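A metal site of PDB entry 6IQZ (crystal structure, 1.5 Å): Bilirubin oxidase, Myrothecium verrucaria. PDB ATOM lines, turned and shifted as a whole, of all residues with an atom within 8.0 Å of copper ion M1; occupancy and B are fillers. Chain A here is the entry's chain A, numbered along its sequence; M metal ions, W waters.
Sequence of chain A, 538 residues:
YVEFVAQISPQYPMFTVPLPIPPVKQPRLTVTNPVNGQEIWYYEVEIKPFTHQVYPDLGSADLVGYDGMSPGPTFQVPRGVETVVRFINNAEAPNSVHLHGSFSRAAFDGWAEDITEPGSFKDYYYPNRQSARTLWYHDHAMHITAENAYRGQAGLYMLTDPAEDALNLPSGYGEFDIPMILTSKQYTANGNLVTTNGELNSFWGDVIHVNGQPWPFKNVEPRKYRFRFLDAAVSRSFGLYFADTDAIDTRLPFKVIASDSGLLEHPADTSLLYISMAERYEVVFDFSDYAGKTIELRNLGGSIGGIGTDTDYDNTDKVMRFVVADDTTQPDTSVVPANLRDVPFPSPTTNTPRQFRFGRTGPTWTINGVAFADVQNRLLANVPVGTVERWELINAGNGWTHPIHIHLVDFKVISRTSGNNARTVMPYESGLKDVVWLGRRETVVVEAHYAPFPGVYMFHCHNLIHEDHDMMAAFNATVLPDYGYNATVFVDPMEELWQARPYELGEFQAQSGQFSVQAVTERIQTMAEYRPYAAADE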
ATOM      1  N   HIS A  98       9.715  13.486 -11.270  1.00  0.00           N
ATOM      2  CA  HIS A  98       9.944  12.934 -12.586  1.00  0.00           C
ATOM      3  C   HIS A  98      11.216  13.509 -13.199  1.00  0.00           C
ATOM      4  O   HIS A  98      11.336  14.740 -13.379  1.00  0.00           O
ATOM      5  CB  HIS A  98       8.765  13.227 -13.502  1.00  0.00           C
ATOM      6  CG  HIS A  98       8.968  12.759 -14.905  1.00  0.00           C
ATOM      7  ND1 HIS A  98       9.457  11.511 -15.219  1.00  0.00           N
ATOM      8  CD2 HIS A  98       8.744  13.378 -16.090  1.00  0.00           C
ATOM      9  CE1 HIS A  98       9.538  11.388 -16.527  1.00  0.00           C
ATOM     10  NE2 HIS A  98       9.110  12.508 -17.079  1.00  0.00           N
ATOM     11  N   LEU A  99      12.179  12.634 -13.503  1.00  0.00           N
ATOM     12  CA  LEU A  99      13.312  13.044 -14.317  1.00  0.00           C
ATOM     13  C   LEU A  99      12.937  12.895 -15.787  1.00  0.00           C
ATOM     14  O   LEU A  99      12.994  11.805 -16.389  1.00  0.00           O
ATOM     15  CB  LEU A  99      14.558  12.236 -13.974  1.00  0.00           C
ATOM     16  CG  LEU A  99      15.828  12.598 -14.764  1.00  0.00           C
ATOM     17  CD1 LEU A  99      16.211  14.063 -14.565  1.00  0.00           C
ATOM     18  CD2 LEU A  99      17.015  11.685 -14.399  1.00  0.00           C
ATOM     19  N   HIS A 100      12.518  14.015 -16.337  1.00  0.00           N
ATOM     20  CA  HIS A 100      12.022  14.094 -17.703  1.00  0.00           C
ATOM     21  C   HIS A 100      13.148  13.986 -18.706  1.00  0.00           C
ATOM     22  O   HIS A 100      14.056  14.826 -18.733  1.00  0.00           O
ATOM     23  CB  HIS A 100      11.277  15.424 -17.848  1.00  0.00           C
ATOM     24  CG  HIS A 100      10.490  15.538 -19.111  1.00  0.00           C
ATOM     25  ND1 HIS A 100       9.201  16.028 -19.143  1.00  0.00           N
ATOM     26  CD2 HIS A 100      10.833  15.287 -20.393  1.00  0.00           C
ATOM     27  CE1 HIS A 100       8.769  16.028 -20.400  1.00  0.00           C
ATOM     28  NE2 HIS A 100       9.750  15.598 -21.176  1.00  0.00           N
ATOM     29  N   GLY A 101      13.083  12.949 -19.533  1.00  0.00           N
ATOM     30  CA  GLY A 101      14.117  12.684 -20.515  1.00  0.00           C
ATOM     31  C   GLY A 101      14.932  11.427 -20.243  1.00  0.00           C
ATOM     32  O   GLY A 101      15.847  11.112 -21.001  1.00  0.00           O
ATOM     33  N   TRP A 136      15.278  17.524 -17.411  1.00  0.00           N
ATOM     34  CA  TRP A 136      14.895  18.359 -16.285  1.00  0.00           C
ATOM     35  C   TRP A 136      14.092  17.510 -15.314  1.00  0.00           C
ATOM     36  O   TRP A 136      13.484  16.515 -15.698  1.00  0.00           O
ATOM     37  CB  TRP A 136      14.131  19.615 -16.741  1.00  0.00           C
ATOM     38  CG  TRP A 136      12.774  19.439 -17.397  1.00  0.00           C
ATOM     39  CD1 TRP A 136      12.468  18.708 -18.531  1.00  0.00           C
ATOM     40  CD2 TRP A 136      11.565  20.077 -16.992  1.00  0.00           C
ATOM     41  NE1 TRP A 136      11.117  18.833 -18.819  1.00  0.00           N
ATOM     42  CE2 TRP A 136      10.547  19.681 -17.903  1.00  0.00           C
ATOM     43  CE3 TRP A 136      11.234  20.958 -15.949  1.00  0.00           C
ATOM     44  CZ2 TRP A 136       9.217  20.128 -17.774  1.00  0.00           C
ATOM     45  CZ3 TRP A 136       9.914  21.391 -15.824  1.00  0.00           C
ATOM     46  CH2 TRP A 136       8.925  20.979 -16.736  1.00  0.00           C
ATOM     47  N   TYR A 137      14.150  17.888 -14.045  1.00  0.00           N
ATOM     48  CA  TYR A 137      13.465  17.125 -13.005  1.00  0.00           C
ATOM     49  C   TYR A 137      12.428  18.042 -12.384  1.00  0.00           C
ATOM     50  O   TYR A 137      12.683  19.232 -12.166  1.00  0.00           O
ATOM     51  CB  TYR A 137      14.465  16.546 -11.982  1.00  0.00           C
ATOM     52  CG  TYR A 137      15.248  17.559 -11.181  1.00  0.00           C
ATOM     53  CD1 TYR A 137      16.318  18.250 -11.733  1.00  0.00           C
ATOM     54  CD2 TYR A 137      14.921  17.816  -9.856  1.00  0.00           C
ATOM     55  CE1 TYR A 137      17.043  19.170 -11.005  1.00  0.00           C
ATOM     56  CE2 TYR A 137      15.634  18.731  -9.116  1.00  0.00           C
ATOM     57  CZ  TYR A 137      16.675  19.420  -9.681  1.00  0.00           C
ATOM     58  OH  TYR A 137      17.388  20.353  -8.926  1.00  0.00           O
ATOM     59  N   HIS A 138      11.226  17.530 -12.171  1.00  0.00           N
ATOM     60  CA  HIS A 138      10.132  18.371 -11.707  1.00  0.00           C
ATOM     61  C   HIS A 138       9.061  17.537 -11.033  1.00  0.00           C
ATOM     62  O   HIS A 138       9.043  16.309 -11.134  1.00  0.00           O
ATOM     63  CB  HIS A 138       9.522  19.166 -12.865  1.00  0.00           C
ATOM     64  CG  HIS A 138       8.869  18.320 -13.921  1.00  0.00           C
ATOM     65  ND1 HIS A 138       7.603  17.796 -13.774  1.00  0.00           N
ATOM     66  CD2 HIS A 138       9.298  17.934 -15.142  1.00  0.00           C
ATOM     67  CE1 HIS A 138       7.284  17.122 -14.859  1.00  0.00           C
ATOM     68  NE2 HIS A 138       8.292  17.185 -15.710  1.00  0.00           N
ATOM     69  N   ASP A 139       8.180  18.210 -10.306  1.00  0.00           N
ATOM     70  CA  ASP A 139       7.169  17.465  -9.590  1.00  0.00           C
ATOM     71  C   ASP A 139       6.103  16.906 -10.507  1.00  0.00           C
ATOM     72  O   ASP A 139       5.811  17.457 -11.566  1.00  0.00           O
ATOM     73  CB  ASP A 139       6.491  18.318  -8.520  1.00  0.00           C
ATOM     74  CG  ASP A 139       5.636  17.475  -7.623  1.00  0.00           C
ATOM     75  OD1 ASP A 139       6.234  16.641  -6.914  1.00  0.00           O
ATOM     76  OD2 ASP A 139       4.397  17.591  -7.663  1.00  0.00           O
ATOM     77  N   HIS A 140       5.524  15.797 -10.048  1.00  0.00           N
ATOM     78  CA  HIS A 140       4.545  15.063 -10.842  1.00  0.00           C
ATOM     79  C   HIS A 140       3.433  14.476  -9.953  1.00  0.00           C
ATOM     80  O   HIS A 140       2.741  13.544 -10.363  1.00  0.00           O
ATOM     81  CB  HIS A 140       5.246  13.940 -11.628  1.00  0.00           C
ATOM     82  CG  HIS A 140       4.704  13.708 -13.006  1.00  0.00           C
ATOM     83  ND1 HIS A 140       3.384  13.419 -13.251  1.00  0.00           N
ATOM     84  CD2 HIS A 140       5.322  13.687 -14.206  1.00  0.00           C
ATOM     85  CE1 HIS A 140       3.200  13.251 -14.551  1.00  0.00           C
ATOM     86  NE2 HIS A 140       4.365  13.401 -15.152  1.00  0.00           N
ATOM     87  N   THR A 145       0.260  18.810  -9.503  1.00  0.00           N
ATOM     88  CA  THR A 145       1.497  19.024 -10.261  1.00  0.00           C
ATOM     89  C   THR A 145       1.639  20.491 -10.693  1.00  0.00           C
ATOM     90  O   THR A 145       2.730  21.053 -10.607  1.00  0.00           O
ATOM     91  CB  THR A 145       1.543  18.093 -11.482  1.00  0.00           C
ATOM     92  OG1 THR A 145       1.656  16.732 -11.022  1.00  0.00           O
ATOM     93  CG2 THR A 145       2.722  18.413 -12.383  1.00  0.00           C
ATOM     94  N   LEU A 230      14.318  25.724 -22.005  1.00  0.00           N
ATOM     95  CA  LEU A 230      13.291  24.825 -21.485  1.00  0.00           C
ATOM     96  C   LEU A 230      12.046  25.636 -21.219  1.00  0.00           C
ATOM     97  O   LEU A 230      12.133  26.686 -20.574  1.00  0.00           O
ATOM     98  CB  LEU A 230      13.750  24.146 -20.184  1.00  0.00           C
ATOM     99  CG  LEU A 230      12.667  23.534 -19.293  1.00  0.00           C
ATOM    100  CD1 LEU A 230      11.967  22.337 -19.945  1.00  0.00           C
ATOM    101  CD2 LEU A 230      13.266  23.145 -17.929  1.00  0.00           C
ATOM    102  N   ASP A 231      10.897  25.179 -21.715  1.00  0.00           N
ATOM    103  CA  ASP A 231       9.620  25.799 -21.341  1.00  0.00           C
ATOM    104  C   ASP A 231       9.087  25.071 -20.115  1.00  0.00           C
ATOM    105  O   ASP A 231       8.503  23.981 -20.220  1.00  0.00           O
ATOM    106  CB  ASP A 231       8.610  25.769 -22.489  1.00  0.00           C
ATOM    107  CG  ASP A 231       7.323  26.503 -22.159  1.00  0.00           C
ATOM    108  OD1 ASP A 231       7.168  26.949 -21.008  1.00  0.00           O
ATOM    109  OD2 ASP A 231       6.453  26.635 -23.039  1.00  0.00           O
ATOM    110  N   MET A 277       5.328  23.548 -23.550  1.00  0.00           N
ATOM    111  CA  MET A 277       5.655  23.085 -22.219  1.00  0.00           C
ATOM    112  C   MET A 277       6.399  21.755 -22.240  1.00  0.00           C
ATOM    113  O   MET A 277       5.967  20.796 -22.913  1.00  0.00           O
ATOM    114  CB  MET A 277       4.391  22.954 -21.359  1.00  0.00           C
ATOM    115  CG  MET A 277       3.717  24.286 -20.978  1.00  0.00           C
ATOM    116  SD  MET A 277       2.839  25.093 -22.342  1.00  0.00           S
ATOM    117  CE  MET A 277       1.353  24.090 -22.444  1.00  0.00           C
ATOM    118  N   ALA A 278       7.529  21.754 -21.542  1.00  0.00           N
ATOM    119  CA  ALA A 278       8.436  20.610 -21.314  1.00  0.00           C
ATOM    120  C   ALA A 278       9.389  20.354 -22.463  1.00  0.00           C
ATOM    121  O   ALA A 278      10.272  19.518 -22.316  1.00  0.00           O
ATOM    122  CB  ALA A 278       7.669  19.340 -20.963  1.00  0.00           C
ATOM    123  N   GLU A 279       9.243  21.078 -23.569  1.00  0.00           N
ATOM    124  CA  GLU A 279      10.224  20.944 -24.640  1.00  0.00           C
ATOM    125  C   GLU A 279      11.541  21.607 -24.282  1.00  0.00           C
ATOM    126  O   GLU A 279      11.575  22.650 -23.616  1.00  0.00           O
ATOM    127  CB  GLU A 279       9.710  21.511 -25.958  1.00  0.00           C
ATOM    128  CG  GLU A 279       8.523  20.741 -26.543  1.00  0.00           C
ATOM    129  CD  GLU A 279       8.154  21.200 -27.942  1.00  0.00           C
ATOM    130  OE1 GLU A 279       7.904  22.412 -28.156  1.00  0.00           O
ATOM    131  OE2 GLU A 279       8.120  20.362 -28.859  1.00  0.00           O
ATOM    132  N   ARG A 280      12.625  20.972 -24.732  1.00  0.00           N
ATOM    133  CA  ARG A 280      13.966  21.534 -24.635  1.00  0.00           C
ATOM    134  C   ARG A 280      14.527  21.693 -26.035  1.00  0.00           C
ATOM    135  O   ARG A 280      14.440  20.788 -26.870  1.00  0.00           O
ATOM    136  CB  ARG A 280      14.900  20.625 -23.817  1.00  0.00           C
ATOM    137  CG  ARG A 280      14.597  20.558 -22.328  1.00  0.00           C
ATOM    138  CD  ARG A 280      13.527  19.512 -22.041  1.00  0.00           C
ATOM    139  NE  ARG A 280      14.035  18.140 -22.140  1.00  0.00           N
ATOM    140  CZ  ARG A 280      13.274  17.087 -22.444  1.00  0.00           C
ATOM    141  NH1 ARG A 280      11.983  17.263 -22.705  1.00  0.00           N
ATOM    142  NH2 ARG A 280      13.807  15.874 -22.504  1.00  0.00           N
ATOM    143  N   HIS A 405       3.601  14.420 -23.895  1.00  0.00           N
ATOM    144  CA  HIS A 405       4.799  13.772 -23.409  1.00  0.00           C
ATOM    145  C   HIS A 405       4.547  12.288 -23.256  1.00  0.00           C
ATOM    146  O   HIS A 405       3.567  11.881 -22.641  1.00  0.00           O
ATOM    147  CB  HIS A 405       5.218  14.406 -22.075  1.00  0.00           C
ATOM    148  CG  HIS A 405       6.398  13.745 -21.430  1.00  0.00           C
ATOM    149  ND1 HIS A 405       7.502  13.324 -22.133  1.00  0.00           N
ATOM    150  CD2 HIS A 405       6.649  13.484 -20.133  1.00  0.00           C
ATOM    151  CE1 HIS A 405       8.375  12.798 -21.290  1.00  0.00           C
ATOM    152  NE2 HIS A 405       7.879  12.893 -20.070  1.00  0.00           N
ATOM    153  N   HIS A 407       6.379   9.031 -21.658  1.00  0.00           N
ATOM    154  CA  HIS A 407       7.523   8.604 -20.848  1.00  0.00           C
ATOM    155  C   HIS A 407       8.234   7.408 -21.500  1.00  0.00           C
ATOM    156  O   HIS A 407       7.763   6.869 -22.496  1.00  0.00           O
ATOM    157  CB  HIS A 407       7.089   8.241 -19.430  1.00  0.00           C
ATOM    158  CG  HIS A 407       6.639   9.408 -18.610  1.00  0.00           C
ATOM    159  ND1 HIS A 407       6.979   9.540 -17.279  1.00  0.00           N
ATOM    160  CD2 HIS A 407       5.854  10.467 -18.898  1.00  0.00           C
ATOM    161  CE1 HIS A 407       6.441  10.641 -16.790  1.00  0.00           C
ATOM    162  NE2 HIS A 407       5.747  11.224 -17.756  1.00  0.00           N
ATOM    163  N   ASP A 434      10.768  13.982 -26.955  1.00  0.00           N
ATOM    164  CA  ASP A 434       9.905  13.240 -26.029  1.00  0.00           C
ATOM    165  C   ASP A 434       8.640  14.040 -25.672  1.00  0.00           C
ATOM    166  O   ASP A 434       7.757  13.531 -24.989  1.00  0.00           O
ATOM    167  CB  ASP A 434      10.652  12.784 -24.752  1.00  0.00           C
ATOM    168  CG  ASP A 434      11.281  13.921 -23.957  1.00  0.00           C
ATOM    169  OD1 ASP A 434      10.701  15.021 -23.892  1.00  0.00           O
ATOM    170  OD2 ASP A 434      12.350  13.706 -23.353  1.00  0.00           O
ATOM    171  N   VAL A 435       8.547  15.254 -26.205  1.00  0.00           N
ATOM    172  CA  VAL A 435       7.326  16.069 -26.139  1.00  0.00           C
ATOM    173  C   VAL A 435       7.061  16.581 -27.544  1.00  0.00           C
ATOM    174  O   VAL A 435       7.998  16.912 -28.260  1.00  0.00           O
ATOM    175  CB  VAL A 435       7.477  17.267 -25.181  1.00  0.00           C
ATOM    176  CG1 VAL A 435       6.190  18.105 -25.155  1.00  0.00           C
ATOM    177  CG2 VAL A 435       7.836  16.769 -23.798  1.00  0.00           C
ATOM    178  N   HIS A 460       0.894  11.943 -21.263  1.00  0.00           N
ATOM    179  CA  HIS A 460      -0.016  13.001 -20.885  1.00  0.00           C
ATOM    180  C   HIS A 460       0.280  14.294 -21.610  1.00  0.00           C
ATOM    181  O   HIS A 460       1.344  14.463 -22.195  1.00  0.00           O
ATOM    182  CB  HIS A 460       0.059  13.253 -19.379  1.00  0.00           C
ATOM    183  CG  HIS A 460       1.445  13.586 -18.905  1.00  0.00           C
ATOM    184  ND1 HIS A 460       1.899  14.880 -18.797  1.00  0.00           N
ATOM    185  CD2 HIS A 460       2.466  12.785 -18.529  1.00  0.00           C
ATOM    186  CE1 HIS A 460       3.149  14.867 -18.361  1.00  0.00           C
ATOM    187  NE2 HIS A 460       3.513  13.610 -18.194  1.00  0.00           N
ATOM    188  N   HIS A 462       1.358  18.112 -21.301  1.00  0.00           N
ATOM    189  CA  HIS A 462       2.235  18.779 -20.341  1.00  0.00           C
ATOM    190  C   HIS A 462       1.843  20.238 -20.074  1.00  0.00           C
ATOM    191  O   HIS A 462       2.601  20.971 -19.454  1.00  0.00           O
ATOM    192  CB  HIS A 462       3.695  18.716 -20.805  1.00  0.00           C
ATOM    193  CG  HIS A 462       4.672  18.436 -19.692  1.00  0.00           C
ATOM    194  ND1 HIS A 462       4.953  19.348 -18.699  1.00  0.00           N
ATOM    195  CD2 HIS A 462       5.427  17.344 -19.435  1.00  0.00           C
ATOM    196  CE1 HIS A 462       5.859  18.831 -17.879  1.00  0.00           C
ATOM    197  NE2 HIS A 462       6.161  17.618 -18.303  1.00  0.00           N
ATOM    198  N   LEU A 464       0.112  21.874 -17.502  1.00  0.00           N
ATOM    199  CA  LEU A 464      -0.071  21.251 -16.206  1.00  0.00           C
ATOM    200  C   LEU A 464      -1.493  21.408 -15.672  1.00  0.00           C
ATOM    201  O   LEU A 464      -1.924  20.589 -14.860  1.00  0.00           O
ATOM    202  CB  LEU A 464       0.937  21.820 -15.211  1.00  0.00           C
ATOM    203  CG  LEU A 464       2.386  21.649 -15.625  1.00  0.00           C
ATOM    204  CD1 LEU A 464       3.286  22.152 -14.509  1.00  0.00           C
ATOM    205  CD2 LEU A 464       2.671  20.196 -15.927  1.00  0.00           C
ATOM    206  N   GLU A 467      -3.184  18.506 -17.405  1.00  0.00           N
ATOM    207  CA  GLU A 467      -2.678  17.285 -16.789  1.00  0.00           C
ATOM    208  C   GLU A 467      -3.371  16.992 -15.448  1.00  0.00           C
ATOM    209  O   GLU A 467      -3.730  15.859 -15.159  1.00  0.00           O
ATOM    210  CB  GLU A 467      -1.159  17.397 -16.620  1.00  0.00           C
ATOM    211  CG  GLU A 467      -0.491  16.181 -16.003  1.00  0.00           C
ATOM    212  CD  GLU A 467       1.002  16.387 -15.826  1.00  0.00           C
ATOM    213  OE1 GLU A 467       1.589  17.170 -16.607  1.00  0.00           O
ATOM    214  OE2 GLU A 467       1.588  15.789 -14.896  1.00  0.00           O
HETATM  215 CU    CU M   1       8.057  16.685 -17.623  1.00  0.00          CU
HETATM  216 CU    CU M   2       8.539  12.664 -18.631  1.00  0.00          CU
HETATM  217 CU    CU M   3       4.887  12.892 -17.073  1.00  0.00          CU
HETATM  218  O   HOH W   1       6.257  14.714 -17.309  1.00  0.00           O
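NE2 of His 100 is in hydrogen-bond range of NH1 of Arg 280, 3.2 Å away.
A ring nitrogen (ND1) of His 405 lies close to a ring nitrogen (NE2) of His 100 (3.3 Å).
O of Trp 136 lies within hydrogen-bond range of N of His 100 (2.8 Å).
O of His 138 is in hydrogen-bond range of N of His 98.
OD1 of Asp 434 sits at hydrogen-bond distance from NE2 of His 100 (2.9 Å).
His 98 touches copper ion M1.
Trp 136 touches copper ion M1.
Of the 24 residues printed, 5 come within 4 Å of copper ion M1.
The nearest printed residue that does not touch copper ion M1 is Ala 278 (4.3 Å).
Copper ion M1 is bound by a ring nitrogen (NE2) of His 138 (2.0 Å), a ring nitrogen (ND1) of His 100 (2.0 Å) and a ring nitrogen (NE2) of His 462 (2.2 Å).
Slightly farther from copper ion M1 lies water W1 (2.7 Å).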
